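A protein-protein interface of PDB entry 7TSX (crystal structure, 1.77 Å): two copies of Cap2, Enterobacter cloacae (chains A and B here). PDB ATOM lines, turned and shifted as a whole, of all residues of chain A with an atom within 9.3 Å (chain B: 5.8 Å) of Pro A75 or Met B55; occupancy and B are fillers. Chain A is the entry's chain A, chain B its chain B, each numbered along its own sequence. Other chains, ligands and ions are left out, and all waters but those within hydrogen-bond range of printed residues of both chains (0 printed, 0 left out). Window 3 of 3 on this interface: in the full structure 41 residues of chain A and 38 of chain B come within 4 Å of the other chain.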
ATOM      1  N   MET A  28      18.623 -22.485  14.427  1.00  0.00           N
ATOM      2  CA  MET A  28      18.880 -23.915  14.558  1.00  0.00           C
ATOM      3  C   MET A  28      17.876 -24.559  15.511  1.00  0.00           C
ATOM      4  O   MET A  28      17.358 -25.655  15.249  1.00  0.00           O
ATOM      5  CB  MET A  28      20.312 -24.148  15.031  1.00  0.00           C
ATOM      6  CG  MET A  28      20.657 -25.612  15.174  1.00  0.00           C
ATOM      7  SD  MET A  28      20.579 -26.526  13.623  1.00  0.00           S
ATOM      8  CE  MET A  28      22.041 -25.862  12.806  1.00  0.00           C
ATOM      9  N   ARG A  29      17.587 -23.894  16.630  1.00  0.00           N
ATOM     10  CA  ARG A  29      16.661 -24.484  17.589  1.00  0.00           C
ATOM     11  C   ARG A  29      15.276 -24.669  16.996  1.00  0.00           C
ATOM     12  O   ARG A  29      14.556 -25.593  17.388  1.00  0.00           O
ATOM     13  CB  ARG A  29      16.591 -23.627  18.853  1.00  0.00           C
ATOM     14  CG  ARG A  29      17.932 -23.619  19.593  1.00  0.00           C
ATOM     15  CD  ARG A  29      17.821 -23.109  21.007  1.00  0.00           C
ATOM     16  NE  ARG A  29      19.135 -22.992  21.626  1.00  0.00           N
ATOM     17  CZ  ARG A  29      19.743 -23.964  22.292  1.00  0.00           C
ATOM     18  NH1 ARG A  29      19.146 -25.124  22.530  1.00  0.00           N
ATOM     19  NH2 ARG A  29      20.949 -23.738  22.802  1.00  0.00           N
ATOM     20  N   VAL A  33      18.304 -26.567   9.909  1.00  0.00           N
ATOM     21  CA  VAL A  33      19.514 -27.349  10.113  1.00  0.00           C
ATOM     22  C   VAL A  33      20.595 -27.056   9.082  1.00  0.00           C
ATOM     23  O   VAL A  33      21.777 -27.314   9.351  1.00  0.00           O
ATOM     24  CB  VAL A  33      19.188 -28.854  10.098  1.00  0.00           C
ATOM     25  CG1 VAL A  33      18.308 -29.214  11.312  1.00  0.00           C
ATOM     26  CG2 VAL A  33      18.488 -29.237   8.815  1.00  0.00           C
ATOM     27  N   GLU A  68      30.428 -25.274  15.383  1.00  0.00           N
ATOM     28  CA  GLU A  68      30.575 -26.354  16.353  1.00  0.00           C
ATOM     29  C   GLU A  68      29.463 -26.318  17.395  1.00  0.00           C
ATOM     30  O   GLU A  68      28.932 -27.364  17.786  1.00  0.00           O
ATOM     31  CB  GLU A  68      31.935 -26.271  17.051  1.00  0.00           C
ATOM     32  CG  GLU A  68      33.099 -26.749  16.223  1.00  0.00           C
ATOM     33  CD  GLU A  68      34.389 -26.823  17.029  1.00  0.00           C
ATOM     34  OE1 GLU A  68      34.328 -27.116  18.245  1.00  0.00           O
ATOM     35  OE2 GLU A  68      35.463 -26.577  16.442  1.00  0.00           O
ATOM     36  N   HIS A  69      29.105 -25.117  17.863  1.00  0.00           N
ATOM     37  CA  HIS A  69      27.997 -24.946  18.797  1.00  0.00           C
ATOM     38  C   HIS A  69      26.667 -25.329  18.154  1.00  0.00           C
ATOM     39  O   HIS A  69      25.898 -26.117  18.715  1.00  0.00           O
ATOM     40  CB  HIS A  69      27.992 -23.480  19.287  1.00  0.00           C
ATOM     41  CG  HIS A  69      26.819 -23.121  20.133  1.00  0.00           C
ATOM     42  ND1 HIS A  69      26.599 -23.669  21.378  1.00  0.00           N
ATOM     43  CD2 HIS A  69      25.789 -22.272  19.905  1.00  0.00           C
ATOM     44  CE1 HIS A  69      25.485 -23.166  21.884  1.00  0.00           C
ATOM     45  NE2 HIS A  69      24.974 -22.317  21.008  1.00  0.00           N
ATOM     46  N   LEU A  70      26.378 -24.781  16.973  1.00  0.00           N
ATOM     47  CA  LEU A  70      25.114 -25.080  16.318  1.00  0.00           C
ATOM     48  C   LEU A  70      24.944 -26.587  16.106  1.00  0.00           C
ATOM     49  O   LEU A  70      23.846 -27.143  16.279  1.00  0.00           O
ATOM     50  CB  LEU A  70      25.055 -24.334  14.987  1.00  0.00           C
ATOM     51  CG  LEU A  70      25.075 -22.810  15.009  1.00  0.00           C
ATOM     52  CD1 LEU A  70      25.066 -22.285  13.586  1.00  0.00           C
ATOM     53  CD2 LEU A  70      23.859 -22.289  15.795  1.00  0.00           C
ATOM     54  N   ASN A  71      26.020 -27.275  15.723  1.00  0.00           N
ATOM     55  CA  ASN A  71      25.896 -28.694  15.428  1.00  0.00           C
ATOM     56  C   ASN A  71      25.730 -29.548  16.676  1.00  0.00           C
ATOM     57  O   ASN A  71      25.494 -30.749  16.560  1.00  0.00           O
ATOM     58  CB  ASN A  71      27.105 -29.139  14.606  1.00  0.00           C
ATOM     59  CG  ASN A  71      26.990 -28.698  13.166  1.00  0.00           C
ATOM     60  OD1 ASN A  71      25.873 -28.522  12.657  1.00  0.00           O
ATOM     61  ND2 ASN A  71      28.122 -28.493  12.507  1.00  0.00           N
ATOM     62  N   ARG A  72      25.831 -28.966  17.865  1.00  0.00           N
ATOM     63  CA  ARG A  72      25.522 -29.665  19.112  1.00  0.00           C
ATOM     64  C   ARG A  72      24.079 -29.452  19.576  1.00  0.00           C
ATOM     65  O   ARG A  72      23.670 -30.009  20.603  1.00  0.00           O
ATOM     66  CB  ARG A  72      26.516 -29.224  20.190  1.00  0.00           C
ATOM     67  CG  ARG A  72      27.837 -29.924  20.092  1.00  0.00           C
ATOM     68  CD  ARG A  72      29.046 -29.156  20.654  1.00  0.00           C
ATOM     69  NE  ARG A  72      30.261 -29.958  20.485  1.00  0.00           N
ATOM     70  CZ  ARG A  72      30.903 -30.144  19.331  1.00  0.00           C
ATOM     71  NH1 ARG A  72      30.554 -29.499  18.228  1.00  0.00           N
ATOM     72  NH2 ARG A  72      31.942 -30.981  19.288  1.00  0.00           N
ATOM     73  N   ILE A  73      23.276 -28.721  18.815  1.00  0.00           N
ATOM     74  CA  ILE A  73      21.917 -28.403  19.245  1.00  0.00           C
ATOM     75  C   ILE A  73      20.920 -29.478  18.828  1.00  0.00           C
ATOM     76  O   ILE A  73      20.090 -29.895  19.642  1.00  0.00           O
ATOM     77  CB  ILE A  73      21.525 -27.010  18.712  1.00  0.00           C
ATOM     78  CG1 ILE A  73      22.417 -25.948  19.355  1.00  0.00           C
ATOM     79  CG2 ILE A  73      20.042 -26.734  18.961  1.00  0.00           C
ATOM     80  CD1 ILE A  73      22.100 -24.521  18.914  1.00  0.00           C
ATOM     81  N   LEU A  74      20.987 -29.955  17.580  1.00  0.00           N
ATOM     82  CA  LEU A  74      20.059 -30.957  17.078  1.00  0.00           C
ATOM     83  C   LEU A  74      20.804 -32.114  16.432  1.00  0.00           C
ATOM     84  O   LEU A  74      21.873 -31.913  15.844  1.00  0.00           O
ATOM     85  CB  LEU A  74      19.104 -30.372  16.028  1.00  0.00           C
ATOM     86  CG  LEU A  74      18.209 -29.191  16.400  1.00  0.00           C
ATOM     87  CD1 LEU A  74      17.476 -28.711  15.157  1.00  0.00           C
ATOM     88  CD2 LEU A  74      17.250 -29.573  17.492  1.00  0.00           C
ATOM     89  N   PRO A  75      20.243 -33.332  16.494  1.00  0.00           N
ATOM     90  CA  PRO A  75      20.938 -34.481  15.885  1.00  0.00           C
ATOM     91  C   PRO A  75      21.161 -34.334  14.391  1.00  0.00           C
ATOM     92  O   PRO A  75      22.109 -34.921  13.861  1.00  0.00           O
ATOM     93  CB  PRO A  75      20.017 -35.672  16.191  1.00  0.00           C
ATOM     94  CG  PRO A  75      19.187 -35.221  17.380  1.00  0.00           C
ATOM     95  CD  PRO A  75      19.014 -33.731  17.216  1.00  0.00           C
ATOM     96  N   ASP A  76      20.297 -33.604  13.686  1.00  0.00           N
ATOM     97  CA  ASP A  76      20.416 -33.439  12.243  1.00  0.00           C
ATOM     98  C   ASP A  76      20.976 -32.076  11.843  1.00  0.00           C
ATOM     99  O   ASP A  76      20.935 -31.729  10.660  1.00  0.00           O
ATOM    100  CB  ASP A  76      19.061 -33.647  11.580  1.00  0.00           C
ATOM    101  CG  ASP A  76      18.522 -35.053  11.795  1.00  0.00           C
ATOM    102  OD1 ASP A  76      19.125 -36.002  11.253  1.00  0.00           O
ATOM    103  OD2 ASP A  76      17.520 -35.212  12.525  1.00  0.00           O
ATOM    104  N   ALA A  77      21.483 -31.295  12.792  1.00  0.00           N
ATOM    105  CA  ALA A  77      22.127 -30.032  12.453  1.00  0.00           C
ATOM    106  C   ALA A  77      23.233 -30.269  11.439  1.00  0.00           C
ATOM    107  O   ALA A  77      24.012 -31.215  11.549  1.00  0.00           O
ATOM    108  CB  ALA A  77      22.703 -29.350  13.699  1.00  0.00           C
ATOM    109  N   SER A  78      23.275 -29.419  10.427  1.00  0.00           N
ATOM    110  CA  SER A  78      24.228 -29.533   9.337  1.00  0.00           C
ATOM    111  C   SER A  78      24.834 -28.178   9.027  1.00  0.00           C
ATOM    112  O   SER A  78      24.896 -27.751   7.876  1.00  0.00           O
ATOM    113  CB  SER A  78      23.572 -30.116   8.084  1.00  0.00           C
ATOM    114  OG  SER A  78      23.015 -31.390   8.357  1.00  0.00           O
ATOM    115  N   ALA A  79      25.280 -27.477  10.064  1.00  0.00           N
ATOM    116  CA  ALA A  79      25.939 -26.193   9.884  1.00  0.00           C
ATOM    117  C   ALA A  79      27.344 -26.376   9.300  1.00  0.00           C
ATOM    118  O   ALA A  79      28.061 -27.336   9.614  1.00  0.00           O
ATOM    119  CB  ALA A  79      25.999 -25.455  11.231  1.00  0.00           C
ATOM    120  N   LEU B  48      15.516 -28.821  24.319  1.00  0.00           N
ATOM    121  CA  LEU B  48      16.547 -28.062  23.620  1.00  0.00           C
ATOM    122  C   LEU B  48      16.000 -27.125  22.553  1.00  0.00           C
ATOM    123  O   LEU B  48      16.718 -26.218  22.113  1.00  0.00           O
ATOM    124  CB  LEU B  48      17.545 -29.018  22.971  1.00  0.00           C
ATOM    125  CG  LEU B  48      18.351 -29.856  23.954  1.00  0.00           C
ATOM    126  CD1 LEU B  48      19.345 -30.743  23.183  1.00  0.00           C
ATOM    127  CD2 LEU B  48      19.069 -29.009  24.956  1.00  0.00           C
ATOM    128  N   LEU B  53      21.071 -24.503  26.711  1.00  0.00           N
ATOM    129  CA  LEU B  53      22.120 -25.514  26.612  1.00  0.00           C
ATOM    130  C   LEU B  53      21.969 -26.341  25.332  1.00  0.00           C
ATOM    131  O   LEU B  53      21.124 -26.060  24.483  1.00  0.00           O
ATOM    132  CB  LEU B  53      22.102 -26.407  27.861  1.00  0.00           C
ATOM    133  CG  LEU B  53      22.374 -25.718  29.193  1.00  0.00           C
ATOM    134  CD1 LEU B  53      22.284 -26.714  30.347  1.00  0.00           C
ATOM    135  CD2 LEU B  53      23.749 -25.038  29.160  1.00  0.00           C
ATOM    136  N   THR B  54      22.841 -27.354  25.184  1.00  0.00           N
ATOM    137  CA  THR B  54      22.868 -28.178  23.977  1.00  0.00           C
ATOM    138  C   THR B  54      22.778 -29.670  24.300  1.00  0.00           C
ATOM    139  O   THR B  54      22.581 -30.060  25.459  1.00  0.00           O
ATOM    140  CB  THR B  54      24.146 -27.938  23.156  1.00  0.00           C
ATOM    141  OG1 THR B  54      25.239 -28.605  23.815  1.00  0.00           O
ATOM    142  CG2 THR B  54      24.460 -26.477  23.010  1.00  0.00           C
ATOM    143  N   MET B  55      22.924 -30.516  23.283  1.00  0.00           N
ATOM    144  CA  MET B  55      22.816 -31.950  23.500  1.00  0.00           C
ATOM    145  C   MET B  55      23.828 -32.468  24.511  1.00  0.00           C
ATOM    146  O   MET B  55      23.596 -33.532  25.104  1.00  0.00           O
ATOM    147  CB  MET B  55      23.003 -32.713  22.183  1.00  0.00           C
ATOM    148  CG  MET B  55      21.870 -32.552  21.187  1.00  0.00           C
ATOM    149  SD  MET B  55      22.019 -33.679  19.806  1.00  0.00           S
ATOM    150  CE  MET B  55      23.430 -33.019  18.923  1.00  0.00           C
ATOM    151  N   THR B  56      24.951 -31.768  24.692  1.00  0.00           N
ATOM    152  CA  THR B  56      25.977 -32.247  25.605  1.00  0.00           C
ATOM    153  C   THR B  56      25.517 -32.206  27.056  1.00  0.00           C
ATOM    154  O   THR B  56      26.175 -32.805  27.909  1.00  0.00           O
ATOM    155  CB  THR B  56      27.276 -31.430  25.466  1.00  0.00           C
ATOM    156  OG1 THR B  56      27.058 -30.059  25.833  1.00  0.00           O
ATOM    157  CG2 THR B  56      27.786 -31.511  24.051  1.00  0.00           C
ATOM    158  N   SER B  57      24.409 -31.528  27.356  1.00  0.00           N
ATOM    159  CA  SER B  57      23.891 -31.476  28.719  1.00  0.00           C
ATOM    160  C   SER B  57      22.673 -32.369  28.911  1.00  0.00           C
ATOM    161  O   SER B  57      22.193 -32.498  30.034  1.00  0.00           O
ATOM    162  CB  SER B  57      23.521 -30.039  29.110  1.00  0.00           C
ATOM    163  OG  SER B  57      24.662 -29.197  29.181  1.00  0.00           O
ATOM    164  N   VAL B  58      22.188 -33.014  27.847  1.00  0.00           N
ATOM    165  CA  VAL B  58      21.022 -33.882  27.964  1.00  0.00           C
ATOM    166  C   VAL B  58      21.339 -35.053  28.881  1.00  0.00           C
ATOM    167  O   VAL B  58      22.370 -35.722  28.738  1.00  0.00           O
ATOM    168  CB  VAL B  58      20.572 -34.364  26.578  1.00  0.00           C
ATOM    169  CG1 VAL B  58      19.572 -35.495  26.712  1.00  0.00           C
ATOM    170  CG2 VAL B  58      19.971 -33.200  25.785  1.00  0.00           C
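The guanidinium group of Arg A29 is in hydrogen-bond range of the backbone carbonyl oxygen of Leu B48 (2.7 Å). NH2 of Arg A29 lies within hydrogen-bond range of O of Leu B53 (2.9 Å). N of Met B55 sits at hydrogen-bond distance from O of Arg A72 (2.8 Å). The backbone nitrogen of Pro A75 sits close to the side-chain sulfur of Met B55, at 3.8 Å.
The backbone carbonyl oxygen (O) of Glu A68 is in hydrogen-bond range of the guanidinium group (NH1) of Arg A72 (2.7 Å). OD1 of Asn A71 sits close to O of Ala A77. The side-chain amide oxygen of Asn A71 is in hydrogen-bond range of the backbone NH of Ala A79. The side-chain hydroxyl (OG1) of Thr B54 sits at hydrogen-bond distance from the side-chain hydroxyl (OG1) of Thr B56 (3.1 Å).
His A69 touches Thr B54. Asn A71 touches Met B55. Arg A72 touches Thr B54. Ile A73 touches Leu B48 (O to CD1, 3.7 Å). Ile A73 touches Met B55. Leu A74 touches Met B55 (O to CE, 3.6 Å).
Of the printed residues of chain B, Pro A75 touches Met B55. Of chain A, only Asn A71, Arg A72, Ile A73, Leu A74 and Pro A75 come within 4 Å of Met B55. Thr B54 touches two residues of chain A. No residue of chain A comes within 4 Å of Thr B56. Printed residues of chain B within 4 Å of His A69: Thr B54 (3.6 Å). Of the printed residues of chain B, Leu A74 touches Met B55 (3.6 Å). The nearest printed residue of chain B that does not touch Asn A71 is Thr B54 (6.9 Å).
Of the 7 printed residues of chain B, 4 touch a printed residue of chain A. Printed residues of chain B that touch a printed residue of chain A: Leu B48, Leu B53, Thr B54 and Met B55. Hydrophobic or aromatic side chains of chain B within 4 Å of the printed part of chain A: Leu B48 and Met B55. Along chain B the printed residues that touch a printed residue of chain A span positions 48 to 55. Among the printed residues, 10 pairs touch across the chains. Among the printed residues, no Asp or Glu carboxylate lies within 4 Å of a Lys or Arg side-chain nitrogen of the other chain.
No position is printed for both chains. Of the 10 pairs that touch across the chains among the printed residues, none has its exchanged pair printed and touching as well.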
